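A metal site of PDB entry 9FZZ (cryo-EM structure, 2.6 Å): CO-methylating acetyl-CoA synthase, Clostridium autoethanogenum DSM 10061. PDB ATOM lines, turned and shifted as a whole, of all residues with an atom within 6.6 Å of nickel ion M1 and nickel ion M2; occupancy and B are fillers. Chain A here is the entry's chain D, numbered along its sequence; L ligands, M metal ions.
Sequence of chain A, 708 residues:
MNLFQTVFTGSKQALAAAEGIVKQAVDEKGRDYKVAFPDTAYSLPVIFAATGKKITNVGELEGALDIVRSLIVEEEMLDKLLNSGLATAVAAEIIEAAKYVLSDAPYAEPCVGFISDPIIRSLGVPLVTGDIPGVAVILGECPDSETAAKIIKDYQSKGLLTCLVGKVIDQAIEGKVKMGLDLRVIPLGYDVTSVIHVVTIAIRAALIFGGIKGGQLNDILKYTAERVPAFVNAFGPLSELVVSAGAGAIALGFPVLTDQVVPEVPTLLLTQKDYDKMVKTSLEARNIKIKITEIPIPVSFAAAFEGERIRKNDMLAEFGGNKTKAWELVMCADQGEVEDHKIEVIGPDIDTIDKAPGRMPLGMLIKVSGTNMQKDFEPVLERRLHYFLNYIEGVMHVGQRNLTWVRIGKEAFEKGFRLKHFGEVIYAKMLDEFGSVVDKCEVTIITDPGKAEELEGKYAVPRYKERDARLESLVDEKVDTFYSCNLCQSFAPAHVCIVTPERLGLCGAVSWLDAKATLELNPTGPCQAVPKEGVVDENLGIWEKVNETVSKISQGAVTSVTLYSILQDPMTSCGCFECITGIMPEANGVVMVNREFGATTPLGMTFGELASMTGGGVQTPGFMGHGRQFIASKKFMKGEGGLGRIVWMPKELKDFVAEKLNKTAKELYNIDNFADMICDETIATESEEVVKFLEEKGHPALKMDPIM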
ATOM      1  N   LEU A 487       1.812 -23.160 -22.421  1.00  0.00           N
ATOM      2  CA  LEU A 487       1.632 -22.575 -21.100  1.00  0.00           C
ATOM      3  C   LEU A 487       1.146 -23.593 -20.079  1.00  0.00           C
ATOM      4  O   LEU A 487       1.383 -23.405 -18.879  1.00  0.00           O
ATOM      5  CB  LEU A 487       0.659 -21.394 -21.182  1.00  0.00           C
ATOM      6  CG  LEU A 487       0.533 -20.517 -19.925  1.00  0.00           C
ATOM      7  CD1 LEU A 487       1.869 -19.884 -19.569  1.00  0.00           C
ATOM      8  CD2 LEU A 487      -0.510 -19.441 -20.160  1.00  0.00           C
ATOM      9  N   CYS A 488       0.482 -24.652 -20.512  1.00  0.00           N
ATOM     10  CA  CYS A 488      -0.026 -25.684 -19.623  1.00  0.00           C
ATOM     11  C   CYS A 488       0.992 -26.791 -19.387  1.00  0.00           C
ATOM     12  O   CYS A 488       0.660 -27.800 -18.758  1.00  0.00           O
ATOM     13  CB  CYS A 488      -1.316 -26.287 -20.176  1.00  0.00           C
ATOM     14  SG  CYS A 488      -2.715 -25.160 -20.170  1.00  0.00           S
ATOM     15  N   PHE A 491       1.917 -28.167 -15.682  1.00  0.00           N
ATOM     16  CA  PHE A 491       1.283 -29.343 -15.095  1.00  0.00           C
ATOM     17  C   PHE A 491       1.066 -30.505 -16.070  1.00  0.00           C
ATOM     18  O   PHE A 491       0.734 -31.603 -15.621  1.00  0.00           O
ATOM     19  CB  PHE A 491      -0.064 -28.974 -14.449  1.00  0.00           C
ATOM     20  CG  PHE A 491      -1.075 -28.420 -15.406  1.00  0.00           C
ATOM     21  CD1 PHE A 491      -1.100 -27.052 -15.691  1.00  0.00           C
ATOM     22  CD2 PHE A 491      -2.004 -29.251 -16.007  1.00  0.00           C
ATOM     23  CE1 PHE A 491      -2.032 -26.521 -16.578  1.00  0.00           C
ATOM     24  CE2 PHE A 491      -2.949 -28.735 -16.894  1.00  0.00           C
ATOM     25  CZ  PHE A 491      -2.962 -27.366 -17.183  1.00  0.00           C
ATOM     26  N   ALA A 492       1.245 -30.290 -17.372  1.00  0.00           N
ATOM     27  CA  ALA A 492       1.102 -31.333 -18.387  1.00  0.00           C
ATOM     28  C   ALA A 492       2.382 -31.328 -19.211  1.00  0.00           C
ATOM     29  O   ALA A 492       2.445 -30.689 -20.268  1.00  0.00           O
ATOM     30  CB  ALA A 492      -0.128 -31.101 -19.261  1.00  0.00           C
ATOM     31  N   HIS A 495       2.094 -31.650 -23.120  1.00  0.00           N
ATOM     32  CA  HIS A 495       1.015 -31.001 -23.853  1.00  0.00           C
ATOM     33  C   HIS A 495       1.520 -29.819 -24.677  1.00  0.00           C
ATOM     34  O   HIS A 495       2.189 -28.930 -24.143  1.00  0.00           O
ATOM     35  CB  HIS A 495      -0.073 -30.520 -22.896  1.00  0.00           C
ATOM     36  CG  HIS A 495      -1.165 -29.740 -23.577  1.00  0.00           C
ATOM     37  ND1 HIS A 495      -1.955 -30.275 -24.558  1.00  0.00           N
ATOM     38  CD2 HIS A 495      -1.561 -28.458 -23.442  1.00  0.00           C
ATOM     39  CE1 HIS A 495      -2.810 -29.368 -24.995  1.00  0.00           C
ATOM     40  NE2 HIS A 495      -2.583 -28.243 -24.325  1.00  0.00           N
ATOM     41  N   CYS A 497      -0.393 -27.087 -27.337  1.00  0.00           N
ATOM     42  CA  CYS A 497      -1.625 -26.617 -27.943  1.00  0.00           C
ATOM     43  C   CYS A 497      -1.317 -25.989 -29.291  1.00  0.00           C
ATOM     44  O   CYS A 497      -0.450 -25.115 -29.385  1.00  0.00           O
ATOM     45  CB  CYS A 497      -2.329 -25.586 -27.058  1.00  0.00           C
ATOM     46  SG  CYS A 497      -3.765 -26.216 -26.180  1.00  0.00           S
ATOM     47  N   LEU A 506      -7.685 -25.046 -26.166  1.00  0.00           N
ATOM     48  CA  LEU A 506      -8.710 -25.768 -25.429  1.00  0.00           C
ATOM     49  C   LEU A 506      -8.967 -25.181 -24.049  1.00  0.00           C
ATOM     50  O   LEU A 506      -9.966 -25.537 -23.418  1.00  0.00           O
ATOM     51  CB  LEU A 506      -8.362 -27.260 -25.324  1.00  0.00           C
ATOM     52  CG  LEU A 506      -6.955 -27.665 -24.904  1.00  0.00           C
ATOM     53  CD1 LEU A 506      -6.897 -27.743 -23.411  1.00  0.00           C
ATOM     54  CD2 LEU A 506      -6.600 -29.015 -25.516  1.00  0.00           C
ATOM     55  N   CYS A 507      -8.111 -24.281 -23.563  1.00  0.00           N
ATOM     56  CA  CYS A 507      -8.439 -23.526 -22.370  1.00  0.00           C
ATOM     57  C   CYS A 507      -9.578 -22.540 -22.625  1.00  0.00           C
ATOM     58  O   CYS A 507     -10.233 -22.110 -21.667  1.00  0.00           O
ATOM     59  CB  CYS A 507      -7.215 -22.777 -21.852  1.00  0.00           C
ATOM     60  SG  CYS A 507      -6.554 -21.601 -23.028  1.00  0.00           S
ATOM     61  N   SER A 573      -4.441 -33.223 -24.372  1.00  0.00           N
ATOM     62  CA  SER A 573      -5.196 -32.296 -23.534  1.00  0.00           C
ATOM     63  C   SER A 573      -4.487 -32.158 -22.201  1.00  0.00           C
ATOM     64  O   SER A 573      -3.829 -33.094 -21.728  1.00  0.00           O
ATOM     65  CB  SER A 573      -6.628 -32.790 -23.269  1.00  0.00           C
ATOM     66  OG  SER A 573      -7.368 -32.921 -24.469  1.00  0.00           O
ATOM     67  N   CYS A 574      -4.584 -30.973 -21.603  1.00  0.00           N
ATOM     68  CA  CYS A 574      -3.920 -30.696 -20.329  1.00  0.00           C
ATOM     69  C   CYS A 574      -4.857 -30.867 -19.145  1.00  0.00           C
ATOM     70  O   CYS A 574      -4.660 -31.763 -18.317  1.00  0.00           O
ATOM     71  CB  CYS A 574      -3.304 -29.293 -20.356  1.00  0.00           C
ATOM     72  SG  CYS A 574      -4.324 -28.069 -21.174  1.00  0.00           S
ATOM     73  N   GLY A 575      -5.951 -30.113 -19.096  1.00  0.00           N
ATOM     74  CA  GLY A 575      -6.808 -30.169 -17.921  1.00  0.00           C
ATOM     75  C   GLY A 575      -7.617 -28.913 -17.673  1.00  0.00           C
ATOM     76  O   GLY A 575      -8.466 -28.872 -16.780  1.00  0.00           O
ATOM     77  N   CYS A 576      -7.378 -27.899 -18.489  1.00  0.00           N
ATOM     78  CA  CYS A 576      -8.152 -26.672 -18.485  1.00  0.00           C
ATOM     79  C   CYS A 576      -9.362 -26.732 -19.397  1.00  0.00           C
ATOM     80  O   CYS A 576     -10.169 -25.791 -19.407  1.00  0.00           O
ATOM     81  CB  CYS A 576      -7.253 -25.501 -18.919  1.00  0.00           C
ATOM     82  SG  CYS A 576      -6.111 -25.993 -20.216  1.00  0.00           S
ATOM     83  N   PHE A 577      -9.538 -27.825 -20.137  1.00  0.00           N
ATOM     84  CA  PHE A 577     -10.587 -27.908 -21.133  1.00  0.00           C
ATOM     85  C   PHE A 577     -11.971 -27.847 -20.481  1.00  0.00           C
ATOM     86  O   PHE A 577     -12.196 -28.429 -19.421  1.00  0.00           O
ATOM     87  CB  PHE A 577     -10.446 -29.181 -21.954  1.00  0.00           C
ATOM     88  CG  PHE A 577     -10.065 -30.390 -21.146  1.00  0.00           C
ATOM     89  CD1 PHE A 577     -11.017 -31.081 -20.409  1.00  0.00           C
ATOM     90  CD2 PHE A 577      -8.743 -30.821 -21.110  1.00  0.00           C
ATOM     91  CE1 PHE A 577     -10.662 -32.192 -19.647  1.00  0.00           C
ATOM     92  CE2 PHE A 577      -8.364 -31.939 -20.350  1.00  0.00           C
ATOM     93  CZ  PHE A 577      -9.340 -32.623 -19.611  1.00  0.00           C
HETATM   94 FE1  LIG L   1      -1.850 -22.277 -24.033  1.00  0.00          FE
HETATM   95 FE2  LIG L   1      -3.197 -24.531 -24.786  1.00  0.00          FE
HETATM   96 FE3  LIG L   1      -4.530 -22.483 -23.563  1.00  0.00          FE
HETATM   97 FE4  LIG L   1      -2.769 -24.010 -22.131  1.00  0.00          FE
HETATM   98  S1  LIG L   1      -4.721 -24.705 -23.100  1.00  0.00           S
HETATM   99  S2  LIG L   1      -2.947 -21.740 -22.107  1.00  0.00           S
HETATM  100  S3  LIG L   1      -1.191 -24.439 -23.712  1.00  0.00           S
HETATM  101  S4  LIG L   1      -3.504 -22.416 -25.597  1.00  0.00           S
HETATM  102 CO1  LG2 L   2       0.108 -21.096 -11.827  1.00  0.00          CO
HETATM  103  N1  LG2 L   2       0.163 -19.259 -12.104  1.00  0.00           N
HETATM  104  N2  LG2 L   2      -1.272 -21.271 -13.172  1.00  0.00           N
HETATM  105  N3  LG2 L   2       0.273 -22.875 -11.389  1.00  0.00           N
HETATM  106  N4  LG2 L   2       1.479 -20.643 -10.555  1.00  0.00           N
HETATM  107  C1  LG2 L   2       0.998 -18.400 -11.218  1.00  0.00           C
HETATM  108  C2  LG2 L   2       0.178 -18.038  -9.954  1.00  0.00           C
HETATM  109  C3  LG2 L   2       1.278 -17.179 -12.179  1.00  0.00           C
HETATM  110  C4  LG2 L   2       1.849 -15.912 -11.506  1.00  0.00           C
HETATM  111  C5  LG2 L   2       2.203 -17.639 -13.353  1.00  0.00           C
HETATM  112  C6  LG2 L   2       2.076 -16.731 -14.589  1.00  0.00           C
HETATM  113  O1  LG2 L   2       1.462 -17.025 -15.616  1.00  0.00           O
HETATM  114  N5  LG2 L   2       2.703 -15.554 -14.503  1.00  0.00           N
HETATM  115  C7  LG2 L   2      -0.137 -16.998 -12.753  1.00  0.00           C
HETATM  116  C8  LG2 L   2      -1.187 -16.230 -11.936  1.00  0.00           C
HETATM  117  C9  LG2 L   2      -1.604 -14.891 -12.579  1.00  0.00           C
HETATM  118  C10 LG2 L   2      -2.894 -14.399 -11.940  1.00  0.00           C
HETATM  119  O2  LG2 L   2      -2.886 -14.007 -10.772  1.00  0.00           O
HETATM  120  N6  LG2 L   2      -4.012 -14.450 -12.662  1.00  0.00           N
HETATM  121  C11 LG2 L   2      -0.555 -18.458 -12.883  1.00  0.00           C
HETATM  122  C12 LG2 L   2      -1.552 -18.909 -13.808  1.00  0.00           C
HETATM  123  C13 LG2 L   2      -2.160 -17.783 -14.597  1.00  0.00           C
HETATM  124  C14 LG2 L   2      -1.899 -20.245 -13.929  1.00  0.00           C
HETATM  125  C15 LG2 L   2      -2.920 -20.834 -14.889  1.00  0.00           C
HETATM  126  C16 LG2 L   2      -4.297 -20.177 -14.754  1.00  0.00           C
HETATM  127  C17 LG2 L   2      -2.320 -20.628 -16.332  1.00  0.00           C
HETATM  128  C18 LG2 L   2      -0.872 -21.028 -16.448  1.00  0.00           C
HETATM  129  O3  LG2 L   2       0.006 -20.272 -16.090  1.00  0.00           O
HETATM  130  N7  LG2 L   2      -0.615 -22.239 -16.967  1.00  0.00           N
HETATM  131  C19 LG2 L   2      -2.872 -22.350 -14.585  1.00  0.00           C
HETATM  132  C20 LG2 L   2      -4.217 -22.972 -14.080  1.00  0.00           C
HETATM  133  C21 LG2 L   2      -5.150 -23.241 -15.273  1.00  0.00           C
HETATM  134  C22 LG2 L   2      -6.499 -23.559 -14.802  1.00  0.00           C
HETATM  135  O4  LG2 L   2      -6.801 -24.704 -14.520  1.00  0.00           O
HETATM  136  N8  LG2 L   2      -7.359 -22.543 -14.726  1.00  0.00           N
HETATM  137  C23 LG2 L   2      -1.797 -22.430 -13.507  1.00  0.00           C
HETATM  138  C24 LG2 L   2      -1.420 -23.608 -12.941  1.00  0.00           C
HETATM  139  C25 LG2 L   2      -0.497 -23.825 -11.966  1.00  0.00           C
HETATM  140  C26 LG2 L   2      -0.086 -25.209 -11.520  1.00  0.00           C
HETATM  141  C27 LG2 L   2       0.692 -25.769 -12.752  1.00  0.00           C
HETATM  142  C28 LG2 L   2      -1.327 -26.082 -11.172  1.00  0.00           C
HETATM  143  C29 LG2 L   2       0.841 -24.923 -10.353  1.00  0.00           C
HETATM  144  C30 LG2 L   2       0.197 -25.132  -8.925  1.00  0.00           C
HETATM  145  C31 LG2 L   2       0.638 -26.425  -8.243  1.00  0.00           C
HETATM  146  C32 LG2 L   2      -0.479 -26.820  -7.259  1.00  0.00           C
HETATM  147  O5  LG2 L   2      -1.162 -25.913  -6.645  1.00  0.00           O
HETATM  148  N9  LG2 L   2      -0.693 -28.072  -7.101  1.00  0.00           N
HETATM  149  C33 LG2 L   2       1.124 -23.441 -10.488  1.00  0.00           C
HETATM  150  C34 LG2 L   2       2.019 -22.766  -9.670  1.00  0.00           C
HETATM  151  C35 LG2 L   2       2.873 -23.568  -8.713  1.00  0.00           C
HETATM  152  C36 LG2 L   2       2.156 -21.339  -9.710  1.00  0.00           C
HETATM  153  C37 LG2 L   2       3.205 -20.458  -8.951  1.00  0.00           C
HETATM  154  C38 LG2 L   2       4.572 -20.930  -9.492  1.00  0.00           C
HETATM  155  C39 LG2 L   2       3.256 -20.489  -7.439  1.00  0.00           C
HETATM  156  C40 LG2 L   2       1.948 -20.854  -6.680  1.00  0.00           C
HETATM  157  C41 LG2 L   2       2.282 -21.660  -5.413  1.00  0.00           C
HETATM  158  O6  LG2 L   2       2.452 -22.867  -5.487  1.00  0.00           O
HETATM  159  N10 LG2 L   2       2.442 -20.979  -4.298  1.00  0.00           N
HETATM  160  C42 LG2 L   2       2.846 -19.069  -9.454  1.00  0.00           C
HETATM  161  C43 LG2 L   2       4.021 -18.068  -9.693  1.00  0.00           C
HETATM  162  C44 LG2 L   2       3.881 -16.748  -8.926  1.00  0.00           C
HETATM  163  O7  LG2 L   2       3.185 -16.633  -7.918  1.00  0.00           O
HETATM  164  N11 LG2 L   2       4.571 -15.746  -9.459  1.00  0.00           N
HETATM  165  C45 LG2 L   2       2.121 -19.323 -10.773  1.00  0.00           C
HETATM  166  C46 LG2 L   2       2.815 -21.635  -3.033  1.00  0.00           C
HETATM  167  C47 LG2 L   2       1.607 -22.014  -2.186  1.00  0.00           C
HETATM  168  C48 LG2 L   2       1.977 -23.097  -1.157  1.00  0.00           C
HETATM  169  O8  LG2 L   2       1.268 -20.801  -1.455  1.00  0.00           O
HETATM  170  O9  LG2 L   2      -1.188 -20.720  -1.949  1.00  0.00           O
HETATM  171  O10 LG2 L   2       0.429 -19.013  -3.088  1.00  0.00           O
HETATM  172  P1  LG2 L   2       0.012 -19.883  -1.886  1.00  0.00           P
HETATM  173  O11 LG2 L   2      -0.077 -18.904  -0.578  1.00  0.00           O
HETATM  174  C49 LG2 L   2       1.014 -18.128  -0.185  1.00  0.00           C
HETATM  175  C50 LG2 L   2       0.527 -16.909   0.547  1.00  0.00           C
HETATM  176  O12 LG2 L   2      -0.654 -16.346   0.040  1.00  0.00           O
HETATM  177  C51 LG2 L   2       0.349 -17.404   2.031  1.00  0.00           C
HETATM  178  O13 LG2 L   2       0.950 -18.664   2.119  1.00  0.00           O
HETATM  179  C52 LG2 L   2       1.779 -18.872   0.971  1.00  0.00           C
HETATM  180  C53 LG2 L   2       3.158 -18.351   1.351  1.00  0.00           C
HETATM  181  O14 LG2 L   2       3.762 -19.365   2.226  1.00  0.00           O
HETATM  182  N12 LG2 L   2      -1.039 -17.521   2.461  1.00  0.00           N
HETATM  183  C54 LG2 L   2      -1.614 -16.726   3.425  1.00  0.00           C
HETATM  184  C55 LG2 L   2      -1.970 -18.379   2.071  1.00  0.00           C
HETATM  185  N13 LG2 L   2      -3.119 -18.191   2.702  1.00  0.00           N
HETATM  186  C56 LG2 L   2      -2.919 -17.137   3.579  1.00  0.00           C
HETATM  187  C57 LG2 L   2      -3.730 -16.472   4.505  1.00  0.00           C
HETATM  188  C58 LG2 L   2      -3.219 -15.413   5.240  1.00  0.00           C
HETATM  189  C59 LG2 L   2      -4.105 -14.696   6.229  1.00  0.00           C
HETATM  190  C60 LG2 L   2      -1.891 -14.995   5.089  1.00  0.00           C
HETATM  191  C61 LG2 L   2      -1.289 -13.893   5.853  1.00  0.00           C
HETATM  192  C62 LG2 L   2      -1.086 -15.668   4.163  1.00  0.00           C
HETATM  193 NI    NI M   1      -5.947 -28.170 -19.683  1.00  0.00          NI
HETATM  194 NI    NI M   2      -4.321 -25.828 -21.302  1.00  0.00          NI
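Nickel ion M1 is bound by N of Cys 576 (1.9 Å), N of Gly 575 (2.0 Å), SG of Cys 574 (2.2 Å) and SG of Cys 576 (2.2 Å).
Leu 506 touches nickel ion M2 (CD1 to NI, 3.8 Å).
The nearest printed residue that does not touch nickel ion M2 is Cys 507 (4.2 Å).
Nickel ion M2 is bound by the side-chain sulfur (SG) of Cys 488 (2.1 Å), the side-chain sulfur (SG) of Cys 576 (2.1 Å), a sulfur (S1) of LIG L1 (2.2 Å) and the side-chain sulfur (SG) of Cys 574 (2.2 Å).
Nickel ion M2 has four donor atoms within binding distance.
NE2 of His 495 sits close to SG of Cys 574 (3.6 Å).
A sulfur (S3) of LIG L1 lies close to the backbone NH of Cys 488 (3.6 Å).
The side-chain sulfur of Cys 488 is bound to an iron atom (FE4) of LIG L1.
N of Cys 507 sits close to S1 of LIG L1 (3.4 Å).
FE3 of LIG L1 is bound by SG of Cys 507, at 2.3 Å.
The side-chain sulfur of Cys 497 is bound to an iron atom (FE2) of LIG L1.
A sulfur (S3) of LIG L1 sits close to the backbone NH (N) of Leu 487, 3.5 Å away.
O of Leu 487 sits at hydrogen-bond distance from N7 of LG2 L2.
CZ of Phe 491 touches nickel ion M1, 3.98 Å away.
Leu 506 touches nickel ion M1 (CD1 to NI, 3.9 Å).
Phe 577 touches nickel ion M1.
Within 4 Å of nickel ion M1: Phe 491, Leu 506, Cys 574, Gly 575, Cys 576 and Phe 577.
The nearest printed residue that does not touch nickel ion M1 is Cys 488 (4.4 Å).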
